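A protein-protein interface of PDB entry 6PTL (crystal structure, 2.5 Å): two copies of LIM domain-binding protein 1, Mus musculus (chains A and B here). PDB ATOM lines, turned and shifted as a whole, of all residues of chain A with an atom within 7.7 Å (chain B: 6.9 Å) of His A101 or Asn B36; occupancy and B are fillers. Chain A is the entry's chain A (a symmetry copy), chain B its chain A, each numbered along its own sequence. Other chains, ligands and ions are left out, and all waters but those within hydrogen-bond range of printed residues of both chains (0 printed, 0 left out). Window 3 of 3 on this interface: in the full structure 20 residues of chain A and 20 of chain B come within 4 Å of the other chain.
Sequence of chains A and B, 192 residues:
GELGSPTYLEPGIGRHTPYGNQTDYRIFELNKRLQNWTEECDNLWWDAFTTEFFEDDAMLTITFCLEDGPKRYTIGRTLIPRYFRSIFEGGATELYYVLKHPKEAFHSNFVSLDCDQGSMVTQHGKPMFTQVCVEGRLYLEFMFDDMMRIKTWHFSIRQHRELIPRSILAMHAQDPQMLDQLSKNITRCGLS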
ATOM      1  N   ASP A  24      23.145   2.560  28.024  1.00  0.00           N
ATOM      2  CA  ASP A  24      22.915   1.639  26.875  1.00  0.00           C
ATOM      3  C   ASP A  24      21.604   2.008  26.161  1.00  0.00           C
ATOM      4  O   ASP A  24      21.427   1.568  25.006  1.00  0.00           O
ATOM      5  CB  ASP A  24      22.965   0.166  27.299  1.00  0.00           C
ATOM      6  CG  ASP A  24      22.127  -0.182  28.517  1.00  0.00           C
ATOM      7  OD1 ASP A  24      21.065   0.444  28.699  1.00  0.00           O
ATOM      8  OD2 ASP A  24      22.547  -1.077  29.274  1.00  0.00           O
ATOM      9  N   VAL A  98      25.677  -3.344  18.759  1.00  0.00           N
ATOM     10  CA  VAL A  98      25.186  -4.339  19.759  1.00  0.00           C
ATOM     11  C   VAL A  98      26.194  -4.380  20.912  1.00  0.00           C
ATOM     12  O   VAL A  98      27.380  -4.649  20.641  1.00  0.00           O
ATOM     13  CB  VAL A  98      24.993  -5.731  19.127  1.00  0.00           C
ATOM     14  CG1 VAL A  98      24.365  -6.714  20.103  1.00  0.00           C
ATOM     15  CG2 VAL A  98      24.181  -5.665  17.841  1.00  0.00           C
ATOM     16  N   LEU A  99      25.735  -4.111  22.139  1.00  0.00           N
ATOM     17  CA  LEU A  99      26.564  -4.112  23.374  1.00  0.00           C
ATOM     18  C   LEU A  99      26.114  -5.264  24.278  1.00  0.00           C
ATOM     19  O   LEU A  99      25.024  -5.162  24.874  1.00  0.00           O
ATOM     20  CB  LEU A  99      26.429  -2.758  24.077  1.00  0.00           C
ATOM     21  CG  LEU A  99      26.813  -1.535  23.242  1.00  0.00           C
ATOM     22  CD1 LEU A  99      26.622  -0.255  24.040  1.00  0.00           C
ATOM     23  CD2 LEU A  99      28.246  -1.636  22.740  1.00  0.00           C
ATOM     24  N   LYS A 100      26.931  -6.320  24.351  1.00  0.00           N
ATOM     25  CA  LYS A 100      26.704  -7.532  25.184  1.00  0.00           C
ATOM     26  C   LYS A 100      27.354  -7.311  26.556  1.00  0.00           C
ATOM     27  O   LYS A 100      28.598  -7.257  26.612  1.00  0.00           O
ATOM     28  CB  LYS A 100      27.275  -8.758  24.464  1.00  0.00           C
ATOM     29  CG  LYS A 100      27.088 -10.101  25.163  1.00  0.00           C
ATOM     30  CD  LYS A 100      25.838 -10.850  24.746  1.00  0.00           C
ATOM     31  CE  LYS A 100      25.981 -12.356  24.839  1.00  0.00           C
ATOM     32  NZ  LYS A 100      26.262 -12.809  26.222  1.00  0.00           N
ATOM     33  N   HIS A 101      26.537  -7.166  27.604  1.00  0.00           N
ATOM     34  CA  HIS A 101      26.955  -7.016  29.027  1.00  0.00           C
ATOM     35  C   HIS A 101      27.858  -5.796  29.208  1.00  0.00           C
ATOM     36  O   HIS A 101      29.000  -5.932  29.642  1.00  0.00           O
ATOM     37  CB  HIS A 101      27.651  -8.293  29.521  1.00  0.00           C
ATOM     38  CG  HIS A 101      26.816  -9.523  29.416  1.00  0.00           C
ATOM     39  ND1 HIS A 101      25.607  -9.654  30.070  1.00  0.00           N
ATOM     40  CD2 HIS A 101      27.019 -10.683  28.755  1.00  0.00           C
ATOM     41  CE1 HIS A 101      25.096 -10.839  29.805  1.00  0.00           C
ATOM     42  NE2 HIS A 101      25.942 -11.489  29.002  1.00  0.00           N
ATOM     43  N   PRO A 102      27.384  -4.568  28.894  1.00  0.00           N
ATOM     44  CA  PRO A 102      28.157  -3.356  29.168  1.00  0.00           C
ATOM     45  C   PRO A 102      28.138  -2.985  30.659  1.00  0.00           C
ATOM     46  O   PRO A 102      27.098  -3.117  31.277  1.00  0.00           O
ATOM     47  CB  PRO A 102      27.441  -2.294  28.324  1.00  0.00           C
ATOM     48  CG  PRO A 102      26.002  -2.762  28.298  1.00  0.00           C
ATOM     49  CD  PRO A 102      26.092  -4.275  28.251  1.00  0.00           C
ATOM     50  N   LYS A 103      29.281  -2.534  31.189  1.00  0.00           N
ATOM     51  CA  LYS A 103      29.449  -2.107  32.605  1.00  0.00           C
ATOM     52  C   LYS A 103      29.312  -0.582  32.689  1.00  0.00           C
ATOM     53  O   LYS A 103      30.148   0.118  32.082  1.00  0.00           O
ATOM     54  CB  LYS A 103      30.802  -2.579  33.149  1.00  0.00           C
ATOM     55  CG  LYS A 103      31.081  -4.066  32.971  1.00  0.00           C
ATOM     56  CD  LYS A 103      32.191  -4.595  33.857  1.00  0.00           C
ATOM     57  CE  LYS A 103      32.256  -6.108  33.874  1.00  0.00           C
ATOM     58  NZ  LYS A 103      33.193  -6.608  34.909  1.00  0.00           N
ATOM     59  N   GLU A 104      28.292  -0.099  33.406  1.00  0.00           N
ATOM     60  CA  GLU A 104      28.002   1.346  33.612  1.00  0.00           C
ATOM     61  C   GLU A 104      28.534   1.774  34.985  1.00  0.00           C
ATOM     62  O   GLU A 104      28.161   1.131  35.986  1.00  0.00           O
ATOM     63  CB  GLU A 104      26.498   1.609  33.511  1.00  0.00           C
ATOM     64  CG  GLU A 104      26.122   3.076  33.636  1.00  0.00           C
ATOM     65  CD  GLU A 104      24.628   3.341  33.711  1.00  0.00           C
ATOM     66  OE1 GLU A 104      23.978   2.795  34.623  1.00  0.00           O
ATOM     67  OE2 GLU A 104      24.118   4.092  32.856  1.00  0.00           O
ATOM     68  N   LEU A 113      30.740   3.802  30.038  1.00  0.00           N
ATOM     69  CA  LEU A 113      30.160   2.544  29.498  1.00  0.00           C
ATOM     70  C   LEU A 113      31.295   1.710  28.893  1.00  0.00           C
ATOM     71  O   LEU A 113      31.864   2.144  27.872  1.00  0.00           O
ATOM     72  CB  LEU A 113      29.088   2.875  28.454  1.00  0.00           C
ATOM     73  CG  LEU A 113      28.173   1.715  28.058  1.00  0.00           C
ATOM     74  CD1 LEU A 113      27.388   1.211  29.261  1.00  0.00           C
ATOM     75  CD2 LEU A 113      27.228   2.121  26.938  1.00  0.00           C
ATOM     76  N   ASP A 114      31.618   0.574  29.521  1.00  0.00           N
ATOM     77  CA  ASP A 114      32.718  -0.341  29.113  1.00  0.00           C
ATOM     78  C   ASP A 114      32.104  -1.675  28.675  1.00  0.00           C
ATOM     79  O   ASP A 114      31.473  -2.340  29.519  1.00  0.00           O
ATOM     80  CB  ASP A 114      33.728  -0.520  30.250  1.00  0.00           C
ATOM     81  CG  ASP A 114      35.070  -1.091  29.817  1.00  0.00           C
ATOM     82  OD1 ASP A 114      35.189  -1.505  28.645  1.00  0.00           O
ATOM     83  OD2 ASP A 114      35.991  -1.113  30.658  1.00  0.00           O
ATOM     84  N   CYS A 115      32.278  -2.035  27.399  1.00  0.00           N
ATOM     85  CA  CYS A 115      31.740  -3.274  26.775  1.00  0.00           C
ATOM     86  C   CYS A 115      32.852  -3.983  25.994  1.00  0.00           C
ATOM     87  O   CYS A 115      33.238  -3.470  24.926  1.00  0.00           O
ATOM     88  CB  CYS A 115      30.568  -2.951  25.854  1.00  0.00           C
ATOM     89  SG  CYS A 115      29.776  -4.422  25.153  1.00  0.00           S
ATOM     90  N   ASP A 116      33.346  -5.110  26.518  1.00  0.00           N
ATOM     91  CA  ASP A 116      34.388  -5.955  25.873  1.00  0.00           C
ATOM     92  C   ASP A 116      33.800  -6.604  24.615  1.00  0.00           C
ATOM     93  O   ASP A 116      34.495  -6.609  23.581  1.00  0.00           O
ATOM     94  CB  ASP A 116      34.938  -7.011  26.838  1.00  0.00           C
ATOM     95  CG  ASP A 116      35.913  -6.469  27.872  1.00  0.00           C
ATOM     96  OD1 ASP A 116      36.458  -5.366  27.655  1.00  0.00           O
ATOM     97  OD2 ASP A 116      36.123  -7.158  28.889  1.00  0.00           O
ATOM     98  N   GLN A 117      32.570  -7.120  24.705  1.00  0.00           N
ATOM     99  CA  GLN A 117      31.864  -7.826  23.601  1.00  0.00           C
ATOM    100  C   GLN A 117      30.946  -6.835  22.873  1.00  0.00           C
ATOM    101  O   GLN A 117      29.710  -6.974  22.984  1.00  0.00           O
ATOM    102  CB  GLN A 117      31.097  -9.027  24.159  1.00  0.00           C
ATOM    103  CG  GLN A 117      31.995 -10.071  24.809  1.00  0.00           C
ATOM    104  CD  GLN A 117      31.203 -11.186  25.447  1.00  0.00           C
ATOM    105  OE1 GLN A 117      31.229 -11.375  26.661  1.00  0.00           O
ATOM    106  NE2 GLN A 117      30.481 -11.931  24.627  1.00  0.00           N
ATOM    107  N   GLY A 118      31.539  -5.872  22.161  1.00  0.00           N
ATOM    108  CA  GLY A 118      30.829  -4.863  21.349  1.00  0.00           C
ATOM    109  C   GLY A 118      30.908  -5.190  19.869  1.00  0.00           C
ATOM    110  O   GLY A 118      32.007  -5.548  19.407  1.00  0.00           O
ATOM    111  N   ASN B  31      15.581  -8.002  24.340  1.00  0.00           N
ATOM    112  CA  ASN B  31      16.864  -8.334  23.663  1.00  0.00           C
ATOM    113  C   ASN B  31      17.981  -8.469  24.706  1.00  0.00           C
ATOM    114  O   ASN B  31      18.853  -9.341  24.522  1.00  0.00           O
ATOM    115  CB  ASN B  31      17.241  -7.288  22.607  1.00  0.00           C
ATOM    116  CG  ASN B  31      16.401  -7.369  21.350  1.00  0.00           C
ATOM    117  OD1 ASN B  31      15.759  -8.384  21.084  1.00  0.00           O
ATOM    118  ND2 ASN B  31      16.404  -6.307  20.563  1.00  0.00           N
ATOM    119  N   LYS B  32      17.950  -7.643  25.758  1.00  0.00           N
ATOM    120  CA  LYS B  32      19.021  -7.562  26.790  1.00  0.00           C
ATOM    121  C   LYS B  32      18.970  -8.796  27.703  1.00  0.00           C
ATOM    122  O   LYS B  32      20.054  -9.287  28.069  1.00  0.00           O
ATOM    123  CB  LYS B  32      18.902  -6.275  27.613  1.00  0.00           C
ATOM    124  CG  LYS B  32      20.235  -5.671  28.028  1.00  0.00           C
ATOM    125  CD  LYS B  32      20.154  -4.771  29.239  1.00  0.00           C
ATOM    126  CE  LYS B  32      21.394  -3.920  29.415  1.00  0.00           C
ATOM    127  NZ  LYS B  32      22.617  -4.745  29.554  1.00  0.00           N
ATOM    128  N   ARG B  33      17.770  -9.265  28.068  1.00  0.00           N
ATOM    129  CA  ARG B  33      17.584 -10.464  28.930  1.00  0.00           C
ATOM    130  C   ARG B  33      18.054 -11.714  28.177  1.00  0.00           C
ATOM    131  O   ARG B  33      18.581 -12.628  28.837  1.00  0.00           O
ATOM    132  CB  ARG B  33      16.122 -10.593  29.371  1.00  0.00           C
ATOM    133  CG  ARG B  33      15.706  -9.585  30.432  1.00  0.00           C
ATOM    134  CD  ARG B  33      16.605  -9.644  31.653  1.00  0.00           C
ATOM    135  NE  ARG B  33      16.516 -10.925  32.340  1.00  0.00           N
ATOM    136  CZ  ARG B  33      15.962 -11.101  33.534  1.00  0.00           C
ATOM    137  NH1 ARG B  33      15.926 -12.305  34.078  1.00  0.00           N
ATOM    138  NH2 ARG B  33      15.448 -10.071  34.182  1.00  0.00           N
ATOM    139  N   LEU B  34      17.863 -11.740  26.853  1.00  0.00           N
ATOM    140  CA  LEU B  34      18.254 -12.879  25.974  1.00  0.00           C
ATOM    141  C   LEU B  34      19.784 -12.967  25.867  1.00  0.00           C
ATOM    142  O   LEU B  34      20.278 -14.049  25.495  1.00  0.00           O
ATOM    143  CB  LEU B  34      17.606 -12.708  24.596  1.00  0.00           C
ATOM    144  CG  LEU B  34      16.088 -12.891  24.559  1.00  0.00           C
ATOM    145  CD1 LEU B  34      15.521 -12.463  23.214  1.00  0.00           C
ATOM    146  CD2 LEU B  34      15.701 -14.330  24.867  1.00  0.00           C
ATOM    147  N   GLN B  35      20.501 -11.880  26.174  1.00  0.00           N
ATOM    148  CA  GLN B  35      21.989 -11.836  26.227  1.00  0.00           C
ATOM    149  C   GLN B  35      22.496 -12.631  27.438  1.00  0.00           C
ATOM    150  O   GLN B  35      23.643 -13.118  27.376  1.00  0.00           O
ATOM    151  CB  GLN B  35      22.488 -10.391  26.294  1.00  0.00           C
ATOM    152  CG  GLN B  35      22.379  -9.643  24.973  1.00  0.00           C
ATOM    153  CD  GLN B  35      22.740  -8.182  25.098  1.00  0.00           C
ATOM    154  OE1 GLN B  35      23.124  -7.701  26.163  1.00  0.00           O
ATOM    155  NE2 GLN B  35      22.619  -7.458  23.997  1.00  0.00           N
ATOM    156  N   ASN B  36      21.681 -12.753  28.493  1.00  0.00           N
ATOM    157  CA  ASN B  36      22.029 -13.464  29.755  1.00  0.00           C
ATOM    158  C   ASN B  36      21.983 -14.985  29.549  1.00  0.00           C
ATOM    159  O   ASN B  36      22.460 -15.702  30.451  1.00  0.00           O
ATOM    160  CB  ASN B  36      21.102 -13.081  30.912  1.00  0.00           C
ATOM    161  CG  ASN B  36      21.178 -11.619  31.297  1.00  0.00           C
ATOM    162  OD1 ASN B  36      22.146 -10.933  30.981  1.00  0.00           O
ATOM    163  ND2 ASN B  36      20.162 -11.134  31.992  1.00  0.00           N
ATOM    164  N   TRP B  37      21.424 -15.465  28.430  1.00  0.00           N
ATOM    165  CA  TRP B  37      21.294 -16.917  28.127  1.00  0.00           C
ATOM    166  C   TRP B  37      22.682 -17.559  28.038  1.00  0.00           C
ATOM    167  O   TRP B  37      23.544 -17.019  27.314  1.00  0.00           O
ATOM    168  CB  TRP B  37      20.494 -17.168  26.842  1.00  0.00           C
ATOM    169  CG  TRP B  37      20.449 -18.617  26.455  1.00  0.00           C
ATOM    170  CD1 TRP B  37      19.525 -19.543  26.844  1.00  0.00           C
ATOM    171  CD2 TRP B  37      21.391 -19.320  25.624  1.00  0.00           C
ATOM    172  NE1 TRP B  37      19.818 -20.767  26.304  1.00  0.00           N
ATOM    173  CE2 TRP B  37      20.957 -20.661  25.550  1.00  0.00           C
ATOM    174  CE3 TRP B  37      22.552 -18.949  24.933  1.00  0.00           C
ATOM    175  CZ2 TRP B  37      21.644 -21.627  24.815  1.00  0.00           C
ATOM    176  CZ3 TRP B  37      23.229 -19.903  24.206  1.00  0.00           C
ATOM    177  CH2 TRP B  37      22.779 -21.224  24.148  1.00  0.00           C
ATOM    178  N   THR B  38      22.869 -18.669  28.758  1.00  0.00           N
ATOM    179  CA  THR B  38      23.998 -19.625  28.616  1.00  0.00           C
ATOM    180  C   THR B  38      23.413 -20.994  28.248  1.00  0.00           C
ATOM    181  O   THR B  38      22.179 -21.150  28.353  1.00  0.00           O
ATOM    182  CB  THR B  38      24.840 -19.687  29.897  1.00  0.00           C
ATOM    183  OG1 THR B  38      24.047 -20.276  30.929  1.00  0.00           O
ATOM    184  CG2 THR B  38      25.331 -18.328  30.347  1.00  0.00           C
ATOM    185  N   CYS B  41      21.215 -22.983  31.007  1.00  0.00           N
ATOM    186  CA  CYS B  41      19.997 -22.233  31.428  1.00  0.00           C
ATOM    187  C   CYS B  41      18.842 -23.213  31.666  1.00  0.00           C
ATOM    188  O   CYS B  41      18.466 -23.931  30.718  1.00  0.00           O
ATOM    189  CB  CYS B  41      19.601 -21.175  30.404  1.00  0.00           C
ATOM    190  SG  CYS B  41      20.355 -19.558  30.724  1.00  0.00           S
ATOM    191  N   TRP B  45      14.347 -20.779  34.200  1.00  0.00           N
ATOM    192  CA  TRP B  45      14.908 -19.504  33.675  1.00  0.00           C
ATOM    193  C   TRP B  45      13.997 -18.948  32.573  1.00  0.00           C
ATOM    194  O   TRP B  45      13.758 -17.725  32.567  1.00  0.00           O
ATOM    195  CB  TRP B  45      16.341 -19.708  33.165  1.00  0.00           C
ATOM    196  CG  TRP B  45      17.042 -18.432  32.815  1.00  0.00           C
ATOM    197  CD1 TRP B  45      17.782 -17.645  33.649  1.00  0.00           C
ATOM    198  CD2 TRP B  45      17.062 -17.784  31.531  1.00  0.00           C
ATOM    199  NE1 TRP B  45      18.263 -16.556  32.974  1.00  0.00           N
ATOM    200  CE2 TRP B  45      17.838 -16.614  31.672  1.00  0.00           C
ATOM    201  CE3 TRP B  45      16.505 -18.076  30.280  1.00  0.00           C
ATOM    202  CZ2 TRP B  45      18.069 -15.743  30.609  1.00  0.00           C
ATOM    203  CZ3 TRP B  45      16.732 -17.213  29.231  1.00  0.00           C
ATOM    204  CH2 TRP B  45      17.504 -16.063  29.395  1.00  0.00           C
ATOM    205  N   GLU B  94      22.766 -16.654  20.102  1.00  0.00           N
ATOM    206  CA  GLU B  94      22.200 -15.292  20.306  1.00  0.00           C
ATOM    207  C   GLU B  94      20.827 -15.208  19.632  1.00  0.00           C
ATOM    208  O   GLU B  94      20.597 -15.953  18.659  1.00  0.00           O
ATOM    209  CB  GLU B  94      23.135 -14.223  19.733  1.00  0.00           C
ATOM    210  CG  GLU B  94      24.543 -14.259  20.309  1.00  0.00           C
ATOM    211  CD  GLU B  94      24.661 -13.853  21.770  1.00  0.00           C
ATOM    212  OE1 GLU B  94      23.874 -12.992  22.213  1.00  0.00           O
ATOM    213  OE2 GLU B  94      25.544 -14.399  22.460  1.00  0.00           O
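OE1 of Gln B35 sits close to O of Leu A99. The side-chain amino group of Lys A100 lies within hydrogen-bond range of the backbone carbonyl oxygen of Gln B35, at 2.9 Å. The backbone carbonyl oxygen (O) of Gln B35 sits at hydrogen-bond distance from a ring nitrogen (NE2) of His A101 (3.3 Å). The side-chain amino group (NZ) of Lys B32 is in salt-bridge range of the side-chain carboxylate (OD2) of Asp A24 (3.7 Å).
The backbone NH (N) of Lys A100 sits at hydrogen-bond distance from the backbone carbonyl oxygen (O) of Gln A117, 3.2 Å away. The side-chain amino group of Lys A100 is in hydrogen-bond range of a ring nitrogen (NE2) of His A101 (3.1 Å). O of Lys A100 lies within hydrogen-bond range of SG of Cys A115 (3.4 Å).
OE2 of Glu B94 touches CE of Lys A100, at 3.2 Å. His A101 touches Asn B36 (CE1 to OD1, 3.2 Å). Lys B32 touches Pro A102.
His A101 touches two residues of chain B. Asn B36 touches one residue of chain A. Of the printed residues of chain A, Gln B35 touches Leu A99 (3.4 Å), Lys A100 (2.9 Å) and His A101 (3.3 Å). Printed residues of chain B within 4 Å of Pro A102: Lys B32. Of the printed residues of chain B, Leu A99 touches Gln B35. Of the printed residues of chain B, Lys A100 touches Gln B35 (2.9 Å) and Glu B94 (3.2 Å). The nearest residue of chain B that does not touch His A101 is Lys B32 (4.9 Å). The nearest residue of chain A that does not touch Asn B36 is Lys A100 (5.1 Å).
Printed residues of chain B that touch a printed residue of chain A: Lys B32, Gln B35, Asn B36 and Glu B94. Of the 14 printed residues of chain A, 5 touch a printed residue of chain B. Printed residues of chain A that touch a printed residue of chain B: Asp A24, Leu A99, Lys A100, His A101 and Pro A102. Hydrophobic or aromatic side chains of chain A within 4 Å of the printed part of chain B: His A101 and Pro A102.
No position is printed for both chains. Of the 7 pairs that touch across the chains among the printed residues, none has its exchanged pair printed and touching as well.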
